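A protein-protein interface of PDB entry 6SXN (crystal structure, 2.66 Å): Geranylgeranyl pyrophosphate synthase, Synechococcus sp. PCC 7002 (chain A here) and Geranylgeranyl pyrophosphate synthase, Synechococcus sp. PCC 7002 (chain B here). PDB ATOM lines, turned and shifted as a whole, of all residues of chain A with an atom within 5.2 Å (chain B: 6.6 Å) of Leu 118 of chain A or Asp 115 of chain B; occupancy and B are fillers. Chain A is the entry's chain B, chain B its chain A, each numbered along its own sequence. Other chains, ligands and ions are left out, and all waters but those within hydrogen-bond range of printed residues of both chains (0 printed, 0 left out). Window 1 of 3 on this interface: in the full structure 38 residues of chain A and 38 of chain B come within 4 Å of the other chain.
A ring nitrogen (NE2) of His 83 of chain B lies within hydrogen-bond range of the backbone carbonyl oxygen of Ile 111 of chain B, 3.0 Å away.
The backbone carbonyl oxygen of Asp 115 of chain B sits at hydrogen-bond distance from the side-chain hydroxyl of Ser 119 of chain B (3.3 Å).
O of Ala 116 of chain B is in hydrogen-bond range of OG of Ser 119 of chain B, 3.2 Å away.
The backbone carbonyl oxygen (O) of Asp 115 of chain A is in hydrogen-bond range of the side-chain hydroxyl (OG) of Ser 119 of chain A (3.3 Å).
The backbone carbonyl oxygen (O) of Ala 116 of chain A lies within hydrogen-bond range of the side-chain hydroxyl (OG) of Ser 119 of chain A.
The backbone carbonyl oxygen of Val 147 of chain A sits at hydrogen-bond distance from the backbone NH of Val 153 of chain A.
Of the 15 printed residues of chain A, 8 touch a printed residue of chain B.
Hydrophobic or aromatic side chains of chain A within 4 Å of the printed part of chain B: Met 79, His 83, Leu 118, Phe 122, Val 147 and Val 153.
Hydrophobic or aromatic side chains of chain B that line the printed part of chain A: Met 79, His 83, Ile 111, Leu 112, Leu 118 and Phe 122.
Printed residues of chain B within 4 Å of Met 79 of chain A: Asp 115 (3.7 Å).
Leu 118 of chain A touches just one residue of chain B: Asp 115 (3.7 Å).
Printed residues of chain B within 4 Å of Val 153 of chain A: Leu 112 (3.5 Å).
Printed residues of chain A within 4 Å of Ile 111 of chain B: His 83 (3.5 Å).
Asp 115 of chain B touches four residues of chain A.
Printed residues of chain A within 4 Å of Phe 122 of chain B: Ser 119 (3.9 Å) and Phe 122 (3.7 Å).
The nearest residue of chain A that does not touch Asp 115 of chain B is Val 153 of chain A (4.2 Å).
The nearest printed residue of chain B that does not touch Phe 122 of chain A is Leu 118 of chain B (5.3 Å).
OD2 of Asp 115 of chain A lies within hydrogen-bond range of ND1 of His 83 of chain B (2.6 Å).
The side-chain carboxylate (OD2) of Asp 115 of chain B is in hydrogen-bond range of a ring nitrogen (ND1) of His 83 of chain A, at 2.7 Å.
The side-chain carboxylate (OD1) of Asp 115 of chain A sits close to the side-chain carboxylate (OD1) of Asp 115 of chain B (3.4 Å).
OD2 of Asp 115 of chain B touches CE of Met 79 of chain A, at 3.7 Å.
His 83 of chain A touches Ile 111 of chain B (ND1 to CG2, 3.5 Å).
Asp 115 of chain A touches Met 79 of chain B.
Leu 118 of chain B touches Asp 115 of chain A (CD2 to O, 3.8 Å).
Leu 118 of chain A touches Asp 115 of chain B (CD2 to O, 3.7 Å).
Ser 119 of chain A touches Phe 122 of chain B (CB to CE2, 3.9 Å).
CB of Ser 119 of chain B touches CE2 of Phe 122 of chain A (3.9 Å).
Phe 122 of chain B touches Phe 122 of chain A (CG to CB, 3.7 Å).
Val 147 of chain A touches Ser 119 of chain B (CG1 to OG, 3.7 Å).
Val 153 of chain A touches Leu 112 of chain B.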
ATOM      1  N   ILE A  76       3.768  18.864   1.405  1.00  0.00           N
ATOM      2  CA  ILE A  76       4.761  19.282   0.432  1.00  0.00           C
ATOM      3  C   ILE A  76       6.024  19.744   1.162  1.00  0.00           C
ATOM      4  O   ILE A  76       7.138  19.311   0.837  1.00  0.00           O
ATOM      5  CB  ILE A  76       4.202  20.347  -0.507  1.00  0.00           C
ATOM      6  CG1 ILE A  76       3.275  19.729  -1.557  1.00  0.00           C
ATOM      7  CG2 ILE A  76       5.322  21.176  -1.129  1.00  0.00           C
ATOM      8  CD1 ILE A  76       2.283  20.733  -2.121  1.00  0.00           C
ATOM      9  N   MET A  79       7.871  16.742   2.452  1.00  0.00           N
ATOM     10  CA  MET A  79       8.594  15.925   1.485  1.00  0.00           C
ATOM     11  C   MET A  79       9.833  16.673   0.986  1.00  0.00           C
ATOM     12  O   MET A  79      10.844  16.047   0.702  1.00  0.00           O
ATOM     13  CB  MET A  79       7.738  15.393   0.325  1.00  0.00           C
ATOM     14  CG  MET A  79       7.204  16.429  -0.631  1.00  0.00           C
ATOM     15  SD  MET A  79       8.389  16.983  -1.929  1.00  0.00           S
ATOM     16  CE  MET A  79       9.312  15.490  -2.253  1.00  0.00           C
ATOM     17  N   HIS A  83      13.502  14.819   1.196  1.00  0.00           N
ATOM     18  CA  HIS A  83      14.379  14.754   0.047  1.00  0.00           C
ATOM     19  C   HIS A  83      15.645  15.562   0.302  1.00  0.00           C
ATOM     20  O   HIS A  83      16.706  15.142  -0.120  1.00  0.00           O
ATOM     21  CB  HIS A  83      13.626  15.194  -1.216  1.00  0.00           C
ATOM     22  CG  HIS A  83      12.787  14.110  -1.797  1.00  0.00           C
ATOM     23  ND1 HIS A  83      12.298  14.179  -3.095  1.00  0.00           N
ATOM     24  CD2 HIS A  83      12.357  12.938  -1.272  1.00  0.00           C
ATOM     25  CE1 HIS A  83      11.590  13.078  -3.350  1.00  0.00           C
ATOM     26  NE2 HIS A  83      11.604  12.296  -2.236  1.00  0.00           N
ATOM     27  N   ALA A 113       8.774   7.881   0.116  1.00  0.00           N
ATOM     28  CA  ALA A 113       7.885   8.499   1.074  1.00  0.00           C
ATOM     29  C   ALA A 113       7.604   9.944   0.647  1.00  0.00           C
ATOM     30  O   ALA A 113       6.470  10.451   0.736  1.00  0.00           O
ATOM     31  CB  ALA A 113       8.470   8.418   2.461  1.00  0.00           C
ATOM     32  N   GLY A 114       8.662  10.605   0.171  1.00  0.00           N
ATOM     33  CA  GLY A 114       8.552  11.964  -0.320  1.00  0.00           C
ATOM     34  C   GLY A 114       7.622  12.032  -1.516  1.00  0.00           C
ATOM     35  O   GLY A 114       6.738  12.895  -1.565  1.00  0.00           O
ATOM     36  N   ASP A 115       7.807  11.082  -2.443  1.00  0.00           N
ATOM     37  CA  ASP A 115       7.009  11.015  -3.658  1.00  0.00           C
ATOM     38  C   ASP A 115       5.538  10.829  -3.319  1.00  0.00           C
ATOM     39  O   ASP A 115       4.693  11.553  -3.854  1.00  0.00           O
ATOM     40  CB  ASP A 115       7.523   9.933  -4.607  1.00  0.00           C
ATOM     41  CG  ASP A 115       8.907  10.227  -5.165  1.00  0.00           C
ATOM     42  OD1 ASP A 115       9.430  11.375  -4.928  1.00  0.00           O
ATOM     43  OD2 ASP A 115       9.455   9.311  -5.836  1.00  0.00           O
ATOM     44  N   ALA A 116       5.274   9.896  -2.401  1.00  0.00           N
ATOM     45  CA  ALA A 116       3.921   9.601  -1.955  1.00  0.00           C
ATOM     46  C   ALA A 116       3.257  10.861  -1.378  1.00  0.00           C
ATOM     47  O   ALA A 116       2.104  11.159  -1.728  1.00  0.00           O
ATOM     48  CB  ALA A 116       3.948   8.479  -0.943  1.00  0.00           C
ATOM     49  N   LEU A 117       3.993  11.606  -0.540  1.00  0.00           N
ATOM     50  CA  LEU A 117       3.450  12.811   0.074  1.00  0.00           C
ATOM     51  C   LEU A 117       3.180  13.874  -0.972  1.00  0.00           C
ATOM     52  O   LEU A 117       2.133  14.521  -0.923  1.00  0.00           O
ATOM     53  CB  LEU A 117       4.404  13.350   1.149  1.00  0.00           C
ATOM     54  CG  LEU A 117       4.441  12.542   2.444  1.00  0.00           C
ATOM     55  CD1 LEU A 117       5.724  12.851   3.194  1.00  0.00           C
ATOM     56  CD2 LEU A 117       3.202  12.819   3.297  1.00  0.00           C
ATOM     57  N   LEU A 118       4.118  14.053  -1.918  1.00  0.00           N
ATOM     58  CA  LEU A 118       3.944  15.077  -2.939  1.00  0.00           C
ATOM     59  C   LEU A 118       2.675  14.787  -3.736  1.00  0.00           C
ATOM     60  O   LEU A 118       1.901  15.696  -3.997  1.00  0.00           O
ATOM     61  CB  LEU A 118       5.186  15.137  -3.829  1.00  0.00           C
ATOM     62  CG  LEU A 118       5.133  16.111  -5.006  1.00  0.00           C
ATOM     63  CD1 LEU A 118       4.662  17.481  -4.553  1.00  0.00           C
ATOM     64  CD2 LEU A 118       6.507  16.215  -5.625  1.00  0.00           C
ATOM     65  N   SER A 119       2.444  13.526  -4.128  1.00  0.00           N
ATOM     66  CA  SER A 119       1.277  13.271  -4.959  1.00  0.00           C
ATOM     67  C   SER A 119       0.023  13.338  -4.092  1.00  0.00           C
ATOM     68  O   SER A 119      -1.029  13.792  -4.532  1.00  0.00           O
ATOM     69  CB  SER A 119       1.359  12.005  -5.743  1.00  0.00           C
ATOM     70  OG  SER A 119       1.666  10.914  -4.901  1.00  0.00           O
ATOM     71  N   TYR A 120       0.155  12.907  -2.834  1.00  0.00           N
ATOM     72  CA  TYR A 120      -1.007  12.869  -1.981  1.00  0.00           C
ATOM     73  C   TYR A 120      -1.473  14.299  -1.716  1.00  0.00           C
ATOM     74  O   TYR A 120      -2.681  14.538  -1.599  1.00  0.00           O
ATOM     75  CB  TYR A 120      -0.716  12.060  -0.726  1.00  0.00           C
ATOM     76  CG  TYR A 120      -1.914  11.744   0.130  1.00  0.00           C
ATOM     77  CD1 TYR A 120      -3.053  11.183  -0.427  1.00  0.00           C
ATOM     78  CD2 TYR A 120      -1.918  12.051   1.493  1.00  0.00           C
ATOM     79  CE1 TYR A 120      -4.167  10.897   0.347  1.00  0.00           C
ATOM     80  CE2 TYR A 120      -3.025  11.773   2.286  1.00  0.00           C
ATOM     81  CZ  TYR A 120      -4.140  11.175   1.713  1.00  0.00           C
ATOM     82  OH  TYR A 120      -5.206  10.926   2.521  1.00  0.00           O
ATOM     83  N   ALA A 121      -0.532  15.252  -1.678  1.00  0.00           N
ATOM     84  CA  ALA A 121      -0.889  16.649  -1.487  1.00  0.00           C
ATOM     85  C   ALA A 121      -1.952  17.080  -2.497  1.00  0.00           C
ATOM     86  O   ALA A 121      -2.990  17.632  -2.143  1.00  0.00           O
ATOM     87  CB  ALA A 121       0.348  17.511  -1.567  1.00  0.00           C
ATOM     88  N   PHE A 122      -1.696  16.808  -3.767  1.00  0.00           N
ATOM     89  CA  PHE A 122      -2.612  17.202  -4.829  1.00  0.00           C
ATOM     90  C   PHE A 122      -3.921  16.423  -4.704  1.00  0.00           C
ATOM     91  O   PHE A 122      -4.990  17.006  -4.799  1.00  0.00           O
ATOM     92  CB  PHE A 122      -1.939  17.015  -6.190  1.00  0.00           C
ATOM     93  CG  PHE A 122      -0.835  18.004  -6.395  1.00  0.00           C
ATOM     94  CD1 PHE A 122      -1.121  19.278  -6.867  1.00  0.00           C
ATOM     95  CD2 PHE A 122       0.483  17.660  -6.159  1.00  0.00           C
ATOM     96  CE1 PHE A 122      -0.112  20.219  -7.047  1.00  0.00           C
ATOM     97  CE2 PHE A 122       1.493  18.601  -6.353  1.00  0.00           C
ATOM     98  CZ  PHE A 122       1.191  19.876  -6.789  1.00  0.00           C
ATOM     99  N   VAL A 147       5.751  24.642  -6.278  1.00  0.00           N
ATOM    100  CA  VAL A 147       6.509  23.496  -5.809  1.00  0.00           C
ATOM    101  C   VAL A 147       7.602  23.134  -6.808  1.00  0.00           C
ATOM    102  O   VAL A 147       8.656  22.640  -6.423  1.00  0.00           O
ATOM    103  CB  VAL A 147       5.574  22.289  -5.615  1.00  0.00           C
ATOM    104  CG1 VAL A 147       6.363  20.987  -5.595  1.00  0.00           C
ATOM    105  CG2 VAL A 147       4.787  22.433  -4.344  1.00  0.00           C
ATOM    106  N   VAL A 153      11.535  23.700  -6.158  1.00  0.00           N
ATOM    107  CA  VAL A 153      12.581  22.868  -6.736  1.00  0.00           C
ATOM    108  C   VAL A 153      13.579  23.757  -7.465  1.00  0.00           C
ATOM    109  O   VAL A 153      14.791  23.549  -7.359  1.00  0.00           O
ATOM    110  CB  VAL A 153      11.998  21.776  -7.649  1.00  0.00           C
ATOM    111  CG1 VAL A 153      13.072  21.110  -8.490  1.00  0.00           C
ATOM    112  CG2 VAL A 153      11.217  20.739  -6.859  1.00  0.00           C
ATOM    113  N   MET B  79       9.046  10.376 -14.324  1.00  0.00           N
ATOM    114  CA  MET B  79       9.649  10.631 -13.022  1.00  0.00           C
ATOM    115  C   MET B  79       9.771   9.330 -12.224  1.00  0.00           C
ATOM    116  O   MET B  79      10.713   9.158 -11.452  1.00  0.00           O
ATOM    117  CB  MET B  79       8.964  11.745 -12.207  1.00  0.00           C
ATOM    118  CG  MET B  79       7.586  11.454 -11.722  1.00  0.00           C
ATOM    119  SD  MET B  79       7.502  10.492 -10.162  1.00  0.00           S
ATOM    120  CE  MET B  79       8.955  11.000  -9.265  1.00  0.00           C
ATOM    121  N   HIS B  83      13.453   8.264 -10.717  1.00  0.00           N
ATOM    122  CA  HIS B  83      13.657   7.905  -9.327  1.00  0.00           C
ATOM    123  C   HIS B  83      14.045   6.434  -9.218  1.00  0.00           C
ATOM    124  O   HIS B  83      14.864   6.073  -8.375  1.00  0.00           O
ATOM    125  CB  HIS B  83      12.403   8.253  -8.510  1.00  0.00           C
ATOM    126  CG  HIS B  83      12.310   9.695  -8.148  1.00  0.00           C
ATOM    127  ND1 HIS B  83      11.458  10.167  -7.172  1.00  0.00           N
ATOM    128  CD2 HIS B  83      12.979  10.773  -8.609  1.00  0.00           C
ATOM    129  CE1 HIS B  83      11.595  11.473  -7.044  1.00  0.00           C
ATOM    130  NE2 HIS B  83      12.540  11.876  -7.908  1.00  0.00           N
ATOM    131  N   ALA B 110      18.638  14.796 -10.303  1.00  0.00           N
ATOM    132  CA  ALA B 110      17.697  13.787 -10.767  1.00  0.00           C
ATOM    133  C   ALA B 110      16.488  13.738  -9.827  1.00  0.00           C
ATOM    134  O   ALA B 110      15.357  13.720 -10.293  1.00  0.00           O
ATOM    135  CB  ALA B 110      18.376  12.443 -10.871  1.00  0.00           C
ATOM    136  N   ILE B 111      16.743  13.725  -8.517  1.00  0.00           N
ATOM    137  CA  ILE B 111      15.679  13.669  -7.531  1.00  0.00           C
ATOM    138  C   ILE B 111      14.753  14.859  -7.756  1.00  0.00           C
ATOM    139  O   ILE B 111      13.536  14.672  -7.874  1.00  0.00           O
ATOM    140  CB  ILE B 111      16.229  13.615  -6.088  1.00  0.00           C
ATOM    141  CG1 ILE B 111      16.884  12.265  -5.796  1.00  0.00           C
ATOM    142  CG2 ILE B 111      15.142  13.938  -5.076  1.00  0.00           C
ATOM    143  CD1 ILE B 111      17.955  12.338  -4.714  1.00  0.00           C
ATOM    144  N   LEU B 112      15.351  16.057  -7.870  1.00  0.00           N
ATOM    145  CA  LEU B 112      14.563  17.271  -8.030  1.00  0.00           C
ATOM    146  C   LEU B 112      13.829  17.266  -9.376  1.00  0.00           C
ATOM    147  O   LEU B 112      12.693  17.738  -9.491  1.00  0.00           O
ATOM    148  CB  LEU B 112      15.454  18.492  -7.854  1.00  0.00           C
ATOM    149  CG  LEU B 112      16.171  18.610  -6.508  1.00  0.00           C
ATOM    150  CD1 LEU B 112      17.205  19.742  -6.532  1.00  0.00           C
ATOM    151  CD2 LEU B 112      15.176  18.761  -5.371  1.00  0.00           C
ATOM    152  N   ALA B 113      14.452  16.695 -10.411  1.00  0.00           N
ATOM    153  CA  ALA B 113      13.815  16.695 -11.714  1.00  0.00           C
ATOM    154  C   ALA B 113      12.536  15.848 -11.672  1.00  0.00           C
ATOM    155  O   ALA B 113      11.507  16.198 -12.258  1.00  0.00           O
ATOM    156  CB  ALA B 113      14.792  16.241 -12.762  1.00  0.00           C
ATOM    157  N   GLY B 114      12.623  14.728 -10.962  1.00  0.00           N
ATOM    158  CA  GLY B 114      11.490  13.841 -10.781  1.00  0.00           C
ATOM    159  C   GLY B 114      10.367  14.546 -10.025  1.00  0.00           C
ATOM    160  O   GLY B 114       9.207  14.490 -10.454  1.00  0.00           O
ATOM    161  N   ASP B 115      10.743  15.255  -8.949  1.00  0.00           N
ATOM    162  CA  ASP B 115       9.801  15.997  -8.137  1.00  0.00           C
ATOM    163  C   ASP B 115       9.074  17.035  -8.986  1.00  0.00           C
ATOM    164  O   ASP B 115       7.838  17.123  -8.948  1.00  0.00           O
ATOM    165  CB  ASP B 115      10.492  16.613  -6.926  1.00  0.00           C
ATOM    166  CG  ASP B 115      11.006  15.581  -5.931  1.00  0.00           C
ATOM    167  OD1 ASP B 115      10.673  14.349  -6.099  1.00  0.00           O
ATOM    168  OD2 ASP B 115      11.724  16.008  -4.975  1.00  0.00           O
ATOM    169  N   ALA B 116       9.857  17.795  -9.770  1.00  0.00           N
ATOM    170  CA  ALA B 116       9.308  18.830 -10.633  1.00  0.00           C
ATOM    171  C   ALA B 116       8.288  18.235 -11.614  1.00  0.00           C
ATOM    172  O   ALA B 116       7.207  18.801 -11.804  1.00  0.00           O
ATOM    173  CB  ALA B 116      10.428  19.528 -11.338  1.00  0.00           C
ATOM    174  N   LEU B 117       8.627  17.087 -12.219  1.00  0.00           N
ATOM    175  CA  LEU B 117       7.732  16.455 -13.179  1.00  0.00           C
ATOM    176  C   LEU B 117       6.454  15.957 -12.510  1.00  0.00           C
ATOM    177  O   LEU B 117       5.361  16.139 -13.042  1.00  0.00           O
ATOM    178  CB  LEU B 117       8.458  15.318 -13.896  1.00  0.00           C
ATOM    179  CG  LEU B 117       9.478  15.757 -14.943  1.00  0.00           C
ATOM    180  CD1 LEU B 117      10.496  14.668 -15.212  1.00  0.00           C
ATOM    181  CD2 LEU B 117       8.756  16.141 -16.222  1.00  0.00           C
ATOM    182  N   LEU B 118       6.590  15.353 -11.324  1.00  0.00           N
ATOM    183  CA  LEU B 118       5.422  14.836 -10.621  1.00  0.00           C
ATOM    184  C   LEU B 118       4.473  15.984 -10.299  1.00  0.00           C
ATOM    185  O   LEU B 118       3.273  15.839 -10.507  1.00  0.00           O
ATOM    186  CB  LEU B 118       5.853  14.130  -9.337  1.00  0.00           C
ATOM    187  CG  LEU B 118       4.734  13.509  -8.500  1.00  0.00           C
ATOM    188  CD1 LEU B 118       3.737  12.742  -9.341  1.00  0.00           C
ATOM    189  CD2 LEU B 118       5.326  12.563  -7.473  1.00  0.00           C
ATOM    190  N   SER B 119       4.989  17.136  -9.838  1.00  0.00           N
ATOM    191  CA  SER B 119       4.066  18.210  -9.498  1.00  0.00           C
ATOM    192  C   SER B 119       3.509  18.838 -10.764  1.00  0.00           C
ATOM    193  O   SER B 119       2.333  19.213 -10.826  1.00  0.00           O
ATOM    194  CB  SER B 119       4.632  19.241  -8.561  1.00  0.00           C
ATOM    195  OG  SER B 119       5.842  19.770  -9.051  1.00  0.00           O
ATOM    196  N   TYR B 120       4.349  18.889 -11.791  1.00  0.00           N
ATOM    197  CA  TYR B 120       3.916  19.541 -13.003  1.00  0.00           C
ATOM    198  C   TYR B 120       2.779  18.741 -13.644  1.00  0.00           C
ATOM    199  O   TYR B 120       1.862  19.324 -14.235  1.00  0.00           O
ATOM    200  CB  TYR B 120       5.117  19.799 -13.906  1.00  0.00           C
ATOM    201  CG  TYR B 120       4.823  20.731 -15.056  1.00  0.00           C
ATOM    202  CD1 TYR B 120       4.187  21.946 -14.861  1.00  0.00           C
ATOM    203  CD2 TYR B 120       5.172  20.367 -16.348  1.00  0.00           C
ATOM    204  CE1 TYR B 120       3.878  22.765 -15.933  1.00  0.00           C
ATOM    205  CE2 TYR B 120       4.880  21.178 -17.425  1.00  0.00           C
ATOM    206  CZ  TYR B 120       4.251  22.388 -17.218  1.00  0.00           C
ATOM    207  OH  TYR B 120       4.002  23.193 -18.279  1.00  0.00           O
ATOM    208  N   PHE B 122       0.260  17.222 -12.249  1.00  0.00           N
ATOM    209  CA  PHE B 122      -1.038  17.632 -11.669  1.00  0.00           C
ATOM    210  C   PHE B 122      -1.426  19.027 -12.146  1.00  0.00           C
ATOM    211  O   PHE B 122      -2.562  19.240 -12.561  1.00  0.00           O
ATOM    212  CB  PHE B 122      -0.954  17.533 -10.155  1.00  0.00           C
ATOM    213  CG  PHE B 122      -0.937  16.117  -9.663  1.00  0.00           C
ATOM    214  CD1 PHE B 122      -2.094  15.371  -9.624  1.00  0.00           C
ATOM    215  CD2 PHE B 122       0.233  15.534  -9.228  1.00  0.00           C
ATOM    216  CE1 PHE B 122      -2.072  14.074  -9.160  1.00  0.00           C
ATOM    217  CE2 PHE B 122       0.249  14.236  -8.759  1.00  0.00           C
ATOM    218  CZ  PHE B 122      -0.902  13.507  -8.737  1.00  0.00           C
